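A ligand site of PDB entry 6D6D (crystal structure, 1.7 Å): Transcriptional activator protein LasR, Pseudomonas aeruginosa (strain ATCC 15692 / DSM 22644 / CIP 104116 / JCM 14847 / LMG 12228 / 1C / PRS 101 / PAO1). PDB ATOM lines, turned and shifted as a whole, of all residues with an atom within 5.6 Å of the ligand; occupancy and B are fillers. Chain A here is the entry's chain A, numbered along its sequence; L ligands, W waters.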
ATOM      1  N   LEU A  36     -16.603  -7.046 -30.769  1.00  0.00           N
ATOM      2  CA  LEU A  36     -16.540  -8.408 -30.260  1.00  0.00           C
ATOM      3  C   LEU A  36     -16.933  -8.434 -28.788  1.00  0.00           C
ATOM      4  O   LEU A  36     -16.398  -7.676 -27.965  1.00  0.00           O
ATOM      5  CB  LEU A  36     -15.139  -9.018 -30.465  1.00  0.00           C
ATOM      6  CG  LEU A  36     -14.906 -10.456 -29.971  1.00  0.00           C
ATOM      7  CD1 LEU A  36     -14.033 -11.226 -30.939  1.00  0.00           C
ATOM      8  CD2 LEU A  36     -14.297 -10.468 -28.576  1.00  0.00           C
ATOM      9  N   PHE A  37     -17.875  -9.311 -28.458  1.00  0.00           N
ATOM     10  CA  PHE A  37     -18.326  -9.528 -27.092  1.00  0.00           C
ATOM     11  C   PHE A  37     -17.905 -10.946 -26.782  1.00  0.00           C
ATOM     12  O   PHE A  37     -18.266 -11.872 -27.503  1.00  0.00           O
ATOM     13  CB  PHE A  37     -19.838  -9.371 -26.982  1.00  0.00           C
ATOM     14  CG  PHE A  37     -20.392  -9.649 -25.605  1.00  0.00           C
ATOM     15  CD1 PHE A  37     -20.812 -10.932 -25.252  1.00  0.00           C
ATOM     16  CD2 PHE A  37     -20.522  -8.630 -24.675  1.00  0.00           C
ATOM     17  CE1 PHE A  37     -21.330 -11.194 -23.989  1.00  0.00           C
ATOM     18  CE2 PHE A  37     -21.046  -8.881 -23.407  1.00  0.00           C
ATOM     19  CZ  PHE A  37     -21.443 -10.164 -23.063  1.00  0.00           C
ATOM     20  N   GLY A  38     -17.099 -11.103 -25.740  1.00  0.00           N
ATOM     21  CA  GLY A  38     -16.577 -12.411 -25.363  1.00  0.00           C
ATOM     22  C   GLY A  38     -16.779 -12.610 -23.884  1.00  0.00           C
ATOM     23  O   GLY A  38     -16.556 -11.690 -23.090  1.00  0.00           O
ATOM     24  N   LEU A  39     -17.197 -13.810 -23.500  1.00  0.00           N
ATOM     25  CA  LEU A  39     -17.477 -14.107 -22.102  1.00  0.00           C
ATOM     26  C   LEU A  39     -17.007 -15.518 -21.771  1.00  0.00           C
ATOM     27  O   LEU A  39     -17.260 -16.468 -22.520  1.00  0.00           O
ATOM     28  CB  LEU A  39     -18.974 -13.972 -21.829  1.00  0.00           C
ATOM     29  CG  LEU A  39     -19.451 -13.585 -20.429  1.00  0.00           C
ATOM     30  CD1 LEU A  39     -18.883 -12.258 -19.978  1.00  0.00           C
ATOM     31  CD2 LEU A  39     -20.970 -13.519 -20.443  1.00  0.00           C
ATOM     32  N   LEU A  40     -16.288 -15.632 -20.665  1.00  0.00           N
ATOM     33  CA  LEU A  40     -15.888 -16.916 -20.118  1.00  0.00           C
ATOM     34  C   LEU A  40     -16.465 -17.078 -18.716  1.00  0.00           C
ATOM     35  O   LEU A  40     -16.670 -16.096 -18.003  1.00  0.00           O
ATOM     36  CB  LEU A  40     -14.364 -17.015 -20.068  1.00  0.00           C
ATOM     37  CG  LEU A  40     -13.612 -17.315 -21.362  1.00  0.00           C
ATOM     38  CD1 LEU A  40     -12.129 -17.076 -21.154  1.00  0.00           C
ATOM     39  CD2 LEU A  40     -13.883 -18.748 -21.786  1.00  0.00           C
ATOM     40  N   TYR A  47      -9.913 -18.850 -23.892  1.00  0.00           N
ATOM     41  CA  TYR A  47     -10.494 -17.804 -24.737  1.00  0.00           C
ATOM     42  C   TYR A  47     -10.980 -18.357 -26.070  1.00  0.00           C
ATOM     43  O   TYR A  47     -12.003 -17.911 -26.592  1.00  0.00           O
ATOM     44  CB  TYR A  47      -9.481 -16.678 -24.940  1.00  0.00           C
ATOM     45  CG  TYR A  47      -9.050 -16.035 -23.638  1.00  0.00           C
ATOM     46  CD1 TYR A  47      -9.851 -15.075 -23.020  1.00  0.00           C
ATOM     47  CD2 TYR A  47      -7.859 -16.385 -23.017  1.00  0.00           C
ATOM     48  CE1 TYR A  47      -9.481 -14.485 -21.817  1.00  0.00           C
ATOM     49  CE2 TYR A  47      -7.478 -15.810 -21.808  1.00  0.00           C
ATOM     50  CZ  TYR A  47      -8.284 -14.855 -21.221  1.00  0.00           C
ATOM     51  OH  TYR A  47      -7.914 -14.273 -20.036  1.00  0.00           O
ATOM     52  N   GLU A  48     -10.239 -19.352 -26.578  1.00  0.00           N
ATOM     53  CA  GLU A  48     -10.555 -20.086 -27.803  1.00  0.00           C
ATOM     54  C   GLU A  48     -12.030 -20.475 -27.882  1.00  0.00           C
ATOM     55  O   GLU A  48     -12.641 -20.436 -28.952  1.00  0.00           O
ATOM     56  CB  GLU A  48      -9.734 -21.382 -27.841  1.00  0.00           C
ATOM     57  CG  GLU A  48      -8.897 -21.587 -29.074  1.00  0.00           C
ATOM     58  CD  GLU A  48      -7.562 -20.856 -28.985  1.00  0.00           C
ATOM     59  OE1 GLU A  48      -7.566 -19.623 -29.142  1.00  0.00           O
ATOM     60  OE2 GLU A  48      -6.530 -21.511 -28.753  1.00  0.00           O
ATOM     61  N   ALA A  50     -14.608 -19.265 -25.780  1.00  0.00           N
ATOM     62  CA  ALA A  50     -15.498 -18.337 -25.109  1.00  0.00           C
ATOM     63  C   ALA A  50     -16.842 -18.233 -25.828  1.00  0.00           C
ATOM     64  O   ALA A  50     -16.964 -18.577 -27.004  1.00  0.00           O
ATOM     65  CB  ALA A  50     -14.857 -16.964 -25.001  1.00  0.00           C
ATOM     66  N   PHE A  51     -17.834 -17.739 -25.107  1.00  0.00           N
ATOM     67  CA  PHE A  51     -19.068 -17.284 -25.720  1.00  0.00           C
ATOM     68  C   PHE A  51     -18.700 -15.983 -26.443  1.00  0.00           C
ATOM     69  O   PHE A  51     -18.296 -15.019 -25.801  1.00  0.00           O
ATOM     70  CB  PHE A  51     -20.149 -17.049 -24.653  1.00  0.00           C
ATOM     71  CG  PHE A  51     -21.392 -16.382 -25.172  1.00  0.00           C
ATOM     72  CD1 PHE A  51     -22.366 -17.121 -25.829  1.00  0.00           C
ATOM     73  CD2 PHE A  51     -21.583 -15.013 -25.015  1.00  0.00           C
ATOM     74  CE1 PHE A  51     -23.511 -16.497 -26.314  1.00  0.00           C
ATOM     75  CE2 PHE A  51     -22.721 -14.380 -25.493  1.00  0.00           C
ATOM     76  CZ  PHE A  51     -23.688 -15.130 -26.155  1.00  0.00           C
ATOM     77  N   ILE A  52     -18.782 -16.000 -27.767  1.00  0.00           N
ATOM     78  CA  ILE A  52     -18.402 -14.833 -28.563  1.00  0.00           C
ATOM     79  C   ILE A  52     -19.545 -14.363 -29.472  1.00  0.00           C
ATOM     80  O   ILE A  52     -20.201 -15.167 -30.162  1.00  0.00           O
ATOM     81  CB  ILE A  52     -17.086 -15.064 -29.349  1.00  0.00           C
ATOM     82  CG1 ILE A  52     -15.935 -15.261 -28.360  1.00  0.00           C
ATOM     83  CG2 ILE A  52     -16.776 -13.868 -30.258  1.00  0.00           C
ATOM     84  CD1 ILE A  52     -14.779 -16.079 -28.891  1.00  0.00           C
ATOM     85  N   TYR A  56     -16.504  -9.091 -36.062  1.00  0.00           N
ATOM     86  CA  TYR A  56     -15.098  -9.156 -36.467  1.00  0.00           C
ATOM     87  C   TYR A  56     -14.975 -10.082 -37.677  1.00  0.00           C
ATOM     88  O   TYR A  56     -15.713 -11.069 -37.781  1.00  0.00           O
ATOM     89  CB  TYR A  56     -14.252  -9.722 -35.325  1.00  0.00           C
ATOM     90  CG  TYR A  56     -13.717  -8.718 -34.324  1.00  0.00           C
ATOM     91  CD1 TYR A  56     -14.265  -7.443 -34.176  1.00  0.00           C
ATOM     92  CD2 TYR A  56     -12.641  -9.061 -33.494  1.00  0.00           C
ATOM     93  CE1 TYR A  56     -13.773  -6.541 -33.232  1.00  0.00           C
ATOM     94  CE2 TYR A  56     -12.144  -8.170 -32.556  1.00  0.00           C
ATOM     95  CZ  TYR A  56     -12.698  -6.912 -32.434  1.00  0.00           C
ATOM     96  OH  TYR A  56     -12.188  -6.040 -31.498  1.00  0.00           O
ATOM     97  N   TRP A  60     -10.028 -13.294 -39.256  1.00  0.00           N
ATOM     98  CA  TRP A  60      -9.269 -12.711 -38.140  1.00  0.00           C
ATOM     99  C   TRP A  60      -9.517 -13.473 -36.836  1.00  0.00           C
ATOM    100  O   TRP A  60      -8.565 -13.821 -36.130  1.00  0.00           O
ATOM    101  CB  TRP A  60      -9.577 -11.208 -37.992  1.00  0.00           C
ATOM    102  CG  TRP A  60      -9.043 -10.614 -36.707  1.00  0.00           C
ATOM    103  CD1 TRP A  60      -9.776 -10.013 -35.725  1.00  0.00           C
ATOM    104  CD2 TRP A  60      -7.672 -10.586 -36.272  1.00  0.00           C
ATOM    105  NE1 TRP A  60      -8.946  -9.608 -34.705  1.00  0.00           N
ATOM    106  CE2 TRP A  60      -7.651  -9.932 -35.015  1.00  0.00           C
ATOM    107  CE3 TRP A  60      -6.470 -11.037 -36.816  1.00  0.00           C
ATOM    108  CZ2 TRP A  60      -6.467  -9.740 -34.290  1.00  0.00           C
ATOM    109  CZ3 TRP A  60      -5.292 -10.837 -36.094  1.00  0.00           C
ATOM    110  CH2 TRP A  60      -5.299 -10.183 -34.849  1.00  0.00           C
ATOM    111  N   ARG A  61     -10.787 -13.740 -36.533  1.00  0.00           N
ATOM    112  CA  ARG A  61     -11.139 -14.521 -35.357  1.00  0.00           C
ATOM    113  C   ARG A  61     -10.414 -15.869 -35.377  1.00  0.00           C
ATOM    114  O   ARG A  61      -9.832 -16.272 -34.372  1.00  0.00           O
ATOM    115  CB  ARG A  61     -12.655 -14.712 -35.261  1.00  0.00           C
ATOM    116  CG  ARG A  61     -13.379 -13.457 -34.776  1.00  0.00           C
ATOM    117  CD  ARG A  61     -14.778 -13.765 -34.255  1.00  0.00           C
ATOM    118  NE  ARG A  61     -14.794 -14.930 -33.366  1.00  0.00           N
ATOM    119  CZ  ARG A  61     -15.868 -15.666 -33.093  1.00  0.00           C
ATOM    120  NH1 ARG A  61     -17.051 -15.349 -33.623  1.00  0.00           N
ATOM    121  NH2 ARG A  61     -15.772 -16.717 -32.291  1.00  0.00           N
ATOM    122  N   TYR A  64      -6.575 -15.258 -34.888  1.00  0.00           N
ATOM    123  CA  TYR A  64      -6.289 -14.916 -33.496  1.00  0.00           C
ATOM    124  C   TYR A  64      -6.179 -16.164 -32.620  1.00  0.00           C
ATOM    125  O   TYR A  64      -5.253 -16.278 -31.831  1.00  0.00           O
ATOM    126  CB  TYR A  64      -7.396 -14.011 -32.978  1.00  0.00           C
ATOM    127  CG  TYR A  64      -7.240 -13.454 -31.576  1.00  0.00           C
ATOM    128  CD1 TYR A  64      -7.509 -14.245 -30.445  1.00  0.00           C
ATOM    129  CD2 TYR A  64      -6.901 -12.110 -31.372  1.00  0.00           C
ATOM    130  CE1 TYR A  64      -7.401 -13.714 -29.165  1.00  0.00           C
ATOM    131  CE2 TYR A  64      -6.800 -11.588 -30.098  1.00  0.00           C
ATOM    132  CZ  TYR A  64      -7.046 -12.388 -28.996  1.00  0.00           C
ATOM    133  OH  TYR A  64      -6.945 -11.870 -27.732  1.00  0.00           O
ATOM    134  N   ASP A  65      -7.138 -17.074 -32.768  1.00  0.00           N
ATOM    135  CA  ASP A  65      -7.136 -18.345 -32.050  1.00  0.00           C
ATOM    136  C   ASP A  65      -5.933 -19.212 -32.417  1.00  0.00           C
ATOM    137  O   ASP A  65      -5.273 -19.750 -31.513  1.00  0.00           O
ATOM    138  CB  ASP A  65      -8.422 -19.127 -32.334  1.00  0.00           C
ATOM    139  CG  ASP A  65      -9.645 -18.524 -31.659  1.00  0.00           C
ATOM    140  OD1 ASP A  65      -9.529 -17.635 -30.782  1.00  0.00           O
ATOM    141  OD2 ASP A  65     -10.748 -18.982 -32.017  1.00  0.00           O
ATOM    142  N   ASP A  73      -2.084 -10.465 -26.694  1.00  0.00           N
ATOM    143  CA  ASP A  73      -2.978  -9.319 -26.769  1.00  0.00           C
ATOM    144  C   ASP A  73      -2.935  -8.514 -25.456  1.00  0.00           C
ATOM    145  O   ASP A  73      -3.321  -9.033 -24.415  1.00  0.00           O
ATOM    146  CB  ASP A  73      -4.386  -9.861 -26.997  1.00  0.00           C
ATOM    147  CG  ASP A  73      -5.442  -8.786 -27.127  1.00  0.00           C
ATOM    148  OD1 ASP A  73      -5.225  -7.620 -26.754  1.00  0.00           O
ATOM    149  OD2 ASP A  73      -6.520  -9.159 -27.607  1.00  0.00           O
ATOM    150  N   THR A  75      -4.804  -6.318 -24.308  1.00  0.00           N
ATOM    151  CA  THR A  75      -6.104  -6.073 -23.724  1.00  0.00           C
ATOM    152  C   THR A  75      -6.569  -7.235 -22.858  1.00  0.00           C
ATOM    153  O   THR A  75      -7.325  -7.034 -21.914  1.00  0.00           O
ATOM    154  CB  THR A  75      -7.176  -5.665 -24.766  1.00  0.00           C
ATOM    155  OG1 THR A  75      -7.551  -6.799 -25.562  1.00  0.00           O
ATOM    156  CG2 THR A  75      -6.650  -4.547 -25.654  1.00  0.00           C
ATOM    157  N   VAL A  76      -6.072  -8.437 -23.170  1.00  0.00           N
ATOM    158  CA  VAL A  76      -6.440  -9.652 -22.407  1.00  0.00           C
ATOM    159  C   VAL A  76      -5.897  -9.592 -20.981  1.00  0.00           C
ATOM    160  O   VAL A  76      -6.652  -9.738 -20.030  1.00  0.00           O
ATOM    161  CB  VAL A  76      -5.992 -10.942 -23.119  1.00  0.00           C
ATOM    162  CG1 VAL A  76      -6.312 -12.159 -22.266  1.00  0.00           C
ATOM    163  CG2 VAL A  76      -6.666 -11.053 -24.465  1.00  0.00           C
ATOM    164  N   CYS A  79      -7.608  -6.938 -18.910  1.00  0.00           N
ATOM    165  CA  CYS A  79      -8.919  -7.351 -18.415  1.00  0.00           C
ATOM    166  C   CYS A  79      -8.856  -8.158 -17.120  1.00  0.00           C
ATOM    167  O   CYS A  79      -9.729  -8.032 -16.258  1.00  0.00           O
ATOM    168  CB  CYS A  79      -9.690  -8.105 -19.502  1.00  0.00           C
ATOM    169  SG  CYS A  79     -10.352  -7.000 -20.779  1.00  0.00           S
ATOM    170  N   TRP A  88      -7.012   1.437 -27.683  1.00  0.00           N
ATOM    171  CA  TRP A  88      -6.016   0.843 -28.567  1.00  0.00           C
ATOM    172  C   TRP A  88      -5.058   1.915 -29.055  1.00  0.00           C
ATOM    173  O   TRP A  88      -5.156   2.396 -30.180  1.00  0.00           O
ATOM    174  CB  TRP A  88      -6.683   0.136 -29.756  1.00  0.00           C
ATOM    175  CG  TRP A  88      -7.736  -0.892 -29.389  1.00  0.00           C
ATOM    176  CD1 TRP A  88      -8.034  -1.376 -28.130  1.00  0.00           C
ATOM    177  CD2 TRP A  88      -8.602  -1.569 -30.296  1.00  0.00           C
ATOM    178  NE1 TRP A  88      -9.052  -2.304 -28.218  1.00  0.00           N
ATOM    179  CE2 TRP A  88      -9.418  -2.441 -29.527  1.00  0.00           C
ATOM    180  CE3 TRP A  88      -8.776  -1.526 -31.683  1.00  0.00           C
ATOM    181  CZ2 TRP A  88     -10.396  -3.260 -30.117  1.00  0.00           C
ATOM    182  CZ3 TRP A  88      -9.746  -2.336 -32.266  1.00  0.00           C
ATOM    183  CH2 TRP A  88     -10.541  -3.196 -31.479  1.00  0.00           C
ATOM    184  N   ILE A  92       0.057   0.792 -25.750  1.00  0.00           N
ATOM    185  CA  ILE A  92      -0.325  -0.505 -25.171  1.00  0.00           C
ATOM    186  C   ILE A  92       0.393  -1.712 -25.807  1.00  0.00           C
ATOM    187  O   ILE A  92       0.435  -2.794 -25.212  1.00  0.00           O
ATOM    188  CB  ILE A  92      -1.858  -0.735 -25.102  1.00  0.00           C
ATOM    189  CG1 ILE A  92      -2.444  -1.067 -26.491  1.00  0.00           C
ATOM    190  CG2 ILE A  92      -2.545   0.474 -24.487  1.00  0.00           C
ATOM    191  CD1 ILE A  92      -3.882  -1.564 -26.457  1.00  0.00           C
ATOM    192  N   TYR A  93       0.974  -1.495 -26.982  1.00  0.00           N
ATOM    193  CA  TYR A  93       1.727  -2.556 -27.679  1.00  0.00           C
ATOM    194  C   TYR A  93       3.211  -2.401 -27.391  1.00  0.00           C
ATOM    195  O   TYR A  93       3.975  -1.891 -28.214  1.00  0.00           O
ATOM    196  CB  TYR A  93       1.426  -2.527 -29.175  1.00  0.00           C
ATOM    197  CG  TYR A  93      -0.048  -2.495 -29.456  1.00  0.00           C
ATOM    198  CD1 TYR A  93      -0.838  -3.628 -29.260  1.00  0.00           C
ATOM    199  CD2 TYR A  93      -0.667  -1.330 -29.918  1.00  0.00           C
ATOM    200  CE1 TYR A  93      -2.201  -3.600 -29.501  1.00  0.00           C
ATOM    201  CE2 TYR A  93      -2.035  -1.298 -30.171  1.00  0.00           C
ATOM    202  CZ  TYR A  93      -2.785  -2.432 -29.963  1.00  0.00           C
ATOM    203  OH  TYR A  93      -4.142  -2.416 -30.209  1.00  0.00           O
ATOM    204  N   PHE A 101       1.148  -8.262 -33.063  1.00  0.00           N
ATOM    205  CA  PHE A 101      -0.307  -8.342 -32.859  1.00  0.00           C
ATOM    206  C   PHE A 101      -1.019  -7.119 -33.449  1.00  0.00           C
ATOM    207  O   PHE A 101      -2.013  -7.277 -34.158  1.00  0.00           O
ATOM    208  CB  PHE A 101      -0.670  -8.500 -31.372  1.00  0.00           C
ATOM    209  CG  PHE A 101      -2.149  -8.391 -31.099  1.00  0.00           C
ATOM    210  CD1 PHE A 101      -3.035  -9.350 -31.591  1.00  0.00           C
ATOM    211  CD2 PHE A 101      -2.663  -7.339 -30.354  1.00  0.00           C
ATOM    212  CE1 PHE A 101      -4.401  -9.243 -31.366  1.00  0.00           C
ATOM    213  CE2 PHE A 101      -4.028  -7.240 -30.092  1.00  0.00           C
ATOM    214  CZ  PHE A 101      -4.897  -8.196 -30.607  1.00  0.00           C
ATOM    215  N   ALA A 105      -3.789  -7.300 -36.433  1.00  0.00           N
ATOM    216  CA  ALA A 105      -5.114  -6.732 -36.184  1.00  0.00           C
ATOM    217  C   ALA A 105      -5.416  -5.603 -37.171  1.00  0.00           C
ATOM    218  O   ALA A 105      -6.540  -5.488 -37.655  1.00  0.00           O
ATOM    219  CB  ALA A 105      -5.215  -6.236 -34.746  1.00  0.00           C
ATOM    220  N   LEU A 110      -8.776  -3.559 -37.977  1.00  0.00           N
ATOM    221  CA  LEU A 110      -9.021  -3.213 -36.591  1.00  0.00           C
ATOM    222  C   LEU A 110      -7.811  -2.472 -36.065  1.00  0.00           C
ATOM    223  O   LEU A 110      -6.833  -3.080 -35.671  1.00  0.00           O
ATOM    224  CB  LEU A 110      -9.339  -4.483 -35.770  1.00  0.00           C
ATOM    225  CG  LEU A 110     -10.521  -5.265 -36.342  1.00  0.00           C
ATOM    226  CD1 LEU A 110     -10.622  -6.678 -35.787  1.00  0.00           C
ATOM    227  CD2 LEU A 110     -11.835  -4.521 -36.113  1.00  0.00           C
ATOM    228  N   THR A 115     -11.235  -1.573 -25.544  1.00  0.00           N
ATOM    229  CA  THR A 115     -11.767  -2.807 -24.956  1.00  0.00           C
ATOM    230  C   THR A 115     -12.231  -2.476 -23.552  1.00  0.00           C
ATOM    231  O   THR A 115     -11.494  -1.884 -22.757  1.00  0.00           O
ATOM    232  CB  THR A 115     -10.689  -3.919 -24.941  1.00  0.00           C
ATOM    233  OG1 THR A 115     -10.294  -4.233 -26.279  1.00  0.00           O
ATOM    234  CG2 THR A 115     -11.241  -5.186 -24.274  1.00  0.00           C
ATOM    235  N   LEU A 125     -15.785 -13.636 -16.747  1.00  0.00           N
ATOM    236  CA  LEU A 125     -14.726 -12.746 -17.218  1.00  0.00           C
ATOM    237  C   LEU A 125     -14.932 -12.542 -18.697  1.00  0.00           C
ATOM    238  O   LEU A 125     -15.035 -13.501 -19.457  1.00  0.00           O
ATOM    239  CB  LEU A 125     -13.348 -13.376 -16.959  1.00  0.00           C
ATOM    240  CG  LEU A 125     -12.111 -12.716 -17.583  1.00  0.00           C
ATOM    241  CD1 LEU A 125     -11.614 -11.598 -16.677  1.00  0.00           C
ATOM    242  CD2 LEU A 125     -11.033 -13.771 -17.767  1.00  0.00           C
ATOM    243  N   GLY A 126     -14.962 -11.288 -19.115  1.00  0.00           N
ATOM    244  CA  GLY A 126     -15.240 -11.021 -20.515  1.00  0.00           C
ATOM    245  C   GLY A 126     -14.633  -9.731 -20.993  1.00  0.00           C
ATOM    246  O   GLY A 126     -13.892  -9.063 -20.275  1.00  0.00           O
ATOM    247  N   ALA A 127     -14.977  -9.403 -22.239  1.00  0.00           N
ATOM    248  CA  ALA A 127     -14.577  -8.136 -22.826  1.00  0.00           C
ATOM    249  C   ALA A 127     -15.557  -7.713 -23.903  1.00  0.00           C
ATOM    250  O   ALA A 127     -16.031  -8.536 -24.706  1.00  0.00           O
ATOM    251  CB  ALA A 127     -13.184  -8.226 -23.406  1.00  0.00           C
ATOM    252  N   SER A 129     -15.095  -5.341 -26.951  1.00  0.00           N
ATOM    253  CA  SER A 129     -14.139  -4.590 -27.781  1.00  0.00           C
ATOM    254  C   SER A 129     -14.900  -3.928 -28.916  1.00  0.00           C
ATOM    255  O   SER A 129     -15.751  -4.553 -29.561  1.00  0.00           O
ATOM    256  CB  SER A 129     -13.076  -5.512 -28.381  1.00  0.00           C
ATOM    257  OG  SER A 129     -12.252  -6.075 -27.371  1.00  0.00           O
HETATM  258  C1  LIG L   1     -10.486 -10.487 -22.278  1.00  0.00           C
HETATM  259  C2  LIG L   1     -11.196 -11.266 -21.370  1.00  0.00           C
HETATM  260  C3  LIG L   1     -12.117 -12.227 -21.809  1.00  0.00           C
HETATM  261  C4  LIG L   1     -12.324 -12.401 -23.171  1.00  0.00           C
HETATM  262  C5  LIG L   1     -11.625 -11.607 -24.086  1.00  0.00           C
HETATM  263  C6  LIG L   1     -11.808 -11.749 -25.568  1.00  0.00           C
HETATM  264  O1  LIG L   1     -12.894 -11.963 -26.096  1.00  0.00           O
HETATM  265  C7  LIG L   1     -10.821 -12.869 -28.384  1.00  0.00           C
HETATM  266  C8  LIG L   1     -10.580 -11.676 -27.729  1.00  0.00           C
HETATM  267  C9  LIG L   1     -10.765 -12.930 -29.770  1.00  0.00           C
HETATM  268  N1  LIG L   1     -13.930 -14.077 -23.914  1.00  0.00           N
HETATM  269  C10 LIG L   1     -13.160 -13.287 -23.562  1.00  0.00           C
HETATM  270  C11 LIG L   1     -10.699 -10.653 -23.643  1.00  0.00           C
HETATM  271  O2  LIG L   1     -10.616 -11.598 -26.370  1.00  0.00           O
HETATM  272  C12 LIG L   1     -10.249 -10.538 -28.449  1.00  0.00           C
HETATM  273  C13 LIG L   1     -10.191 -10.586 -29.841  1.00  0.00           C
HETATM  274  C14 LIG L   1     -10.440 -11.785 -30.494  1.00  0.00           C
HETATM  275 BR1  LIG L   1     -10.358 -11.876 -32.367  1.00  0.00          BR
HETATM  276 BR2  LIG L   1     -11.247 -14.431 -27.400  1.00  0.00          BR
HETATM  277  C15 LIG L   1      -9.988  -9.260 -27.676  1.00  0.00           C
HETATM  278  N2  LIG L   1      -9.118  -8.282 -28.335  1.00  0.00           N
HETATM  279  C16 LIG L   1      -9.453  -7.394 -29.264  1.00  0.00           C
HETATM  280  O3  LIG L   1     -10.593  -7.316 -29.711  1.00  0.00           O
HETATM  281  C17 LIG L   1      -8.441  -6.416 -29.785  1.00  0.00           C
HETATM  282  C18 LIG L   1      -7.850  -5.547 -28.876  1.00  0.00           C
HETATM  283  C19 LIG L   1      -6.916  -4.604 -29.310  1.00  0.00           C
HETATM  284  C20 LIG L   1      -6.580  -4.518 -30.648  1.00  0.00           C
HETATM  285  C21 LIG L   1      -7.163  -5.381 -31.559  1.00  0.00           C
HETATM  286  C22 LIG L   1      -8.102  -6.322 -31.137  1.00  0.00           C
HETATM  287  N3  LIG L   1      -8.630  -7.196 -32.106  1.00  0.00           N
HETATM  288  O4  LIG L   1      -8.836  -6.738 -33.389  1.00  0.00           O
HETATM  289  O5  LIG L   1      -8.846  -8.371 -31.832  1.00  0.00           O
HETATM  290  O   HOH W   1      -8.751 -11.607 -19.518  1.00  0.00           O
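The backbone NH (N) of Leu 39 lies within hydrogen-bond range of a nitrogen (N1) of the ligand. A nitrogen (N2) of the ligand is in hydrogen-bond range of the side-chain carboxylate of Asp 73 (2.8 Å). The indole nitrogen of Trp 60 lies within hydrogen-bond range of an oxygen (O5) of the ligand, at 3.1 Å. The side-chain hydroxyl (OG) of Ser 129 sits at hydrogen-bond distance from an oxygen (O3) of the ligand, at 3.1 Å. The side-chain hydroxyl of Tyr 56 lies within hydrogen-bond range of an oxygen (O3) of the ligand.
The backbone carbonyl oxygen of Thr 75 lies within hydrogen-bond range of the side-chain sulfur of Cys 79, at 3.2 Å. The side-chain carboxylate (OD1) of Asp 73 lies within hydrogen-bond range of the side-chain hydroxyl (OG1) of Thr 75. The side-chain hydroxyl (OG1) of Thr 115 is in hydrogen-bond range of the indole nitrogen (NE1) of Trp 88 (3.0 Å). The backbone NH (N) of Ala 127 is in hydrogen-bond range of the backbone carbonyl oxygen (O) of Gly 38 (2.9 Å). The backbone NH of Leu 110 sits at hydrogen-bond distance from the backbone carbonyl oxygen of Ala 105, 3.0 Å away. OH of Tyr 64 sits at hydrogen-bond distance from OD2 of Asp 73 (2.7 Å). OG1 of Thr 115 lies within hydrogen-bond range of OG of Ser 129, 2.9 Å away. The backbone carbonyl oxygen (O) of Leu 125 sits at hydrogen-bond distance from the backbone NH (N) of Leu 40 (2.8 Å).
Leu 36 touches the ligand. Gly 38 touches the ligand. CE1 of Tyr 47 touches C3 of the ligand, at 3.5 Å. CB of Ala 50 touches N1 of the ligand, 3.2 Å away. Tyr 64 touches the ligand (CE1 to C9, 3.5 Å). Thr 75 touches the ligand (OG1 to N2, 3.5 Å). Cys 79 touches the ligand (CB to C1, 3.7 Å). Trp 88 touches the ligand. OH of Tyr 93 touches C20 of the ligand, 3.2 Å away. CZ of Phe 101 touches C21 of the ligand, at 3.7 Å. Ala 105 touches the ligand (CB to C21, 3.8 Å). CD1 of Leu 110 touches O4 of the ligand (3.0 Å). Thr 115 touches the ligand (OG1 to C18, 3.8 Å). O of Leu 125 touches C3 of the ligand, 3.96 Å away. CA of Gly 126 touches C3 of the ligand, 3.6 Å away. Ala 127 touches the ligand (CB to C11, 3.5 Å). Hydrophobic or aromatic side chains within 4 Å of the ligand: Leu 36, Tyr 47, Ala 50, Tyr 56, Trp 60, Tyr 64, Trp 88, Phe 101, Ala 105, Leu 110 and Ala 127. Of the 30 residues printed, 21 come within 4 Å of the ligand. The nearest printed residue that does not touch the ligand is Arg 61 (4.1 Å).
Water W1 bridges OH of Tyr 47 (2.8 Å) and O of Val 76 (2.9 Å).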
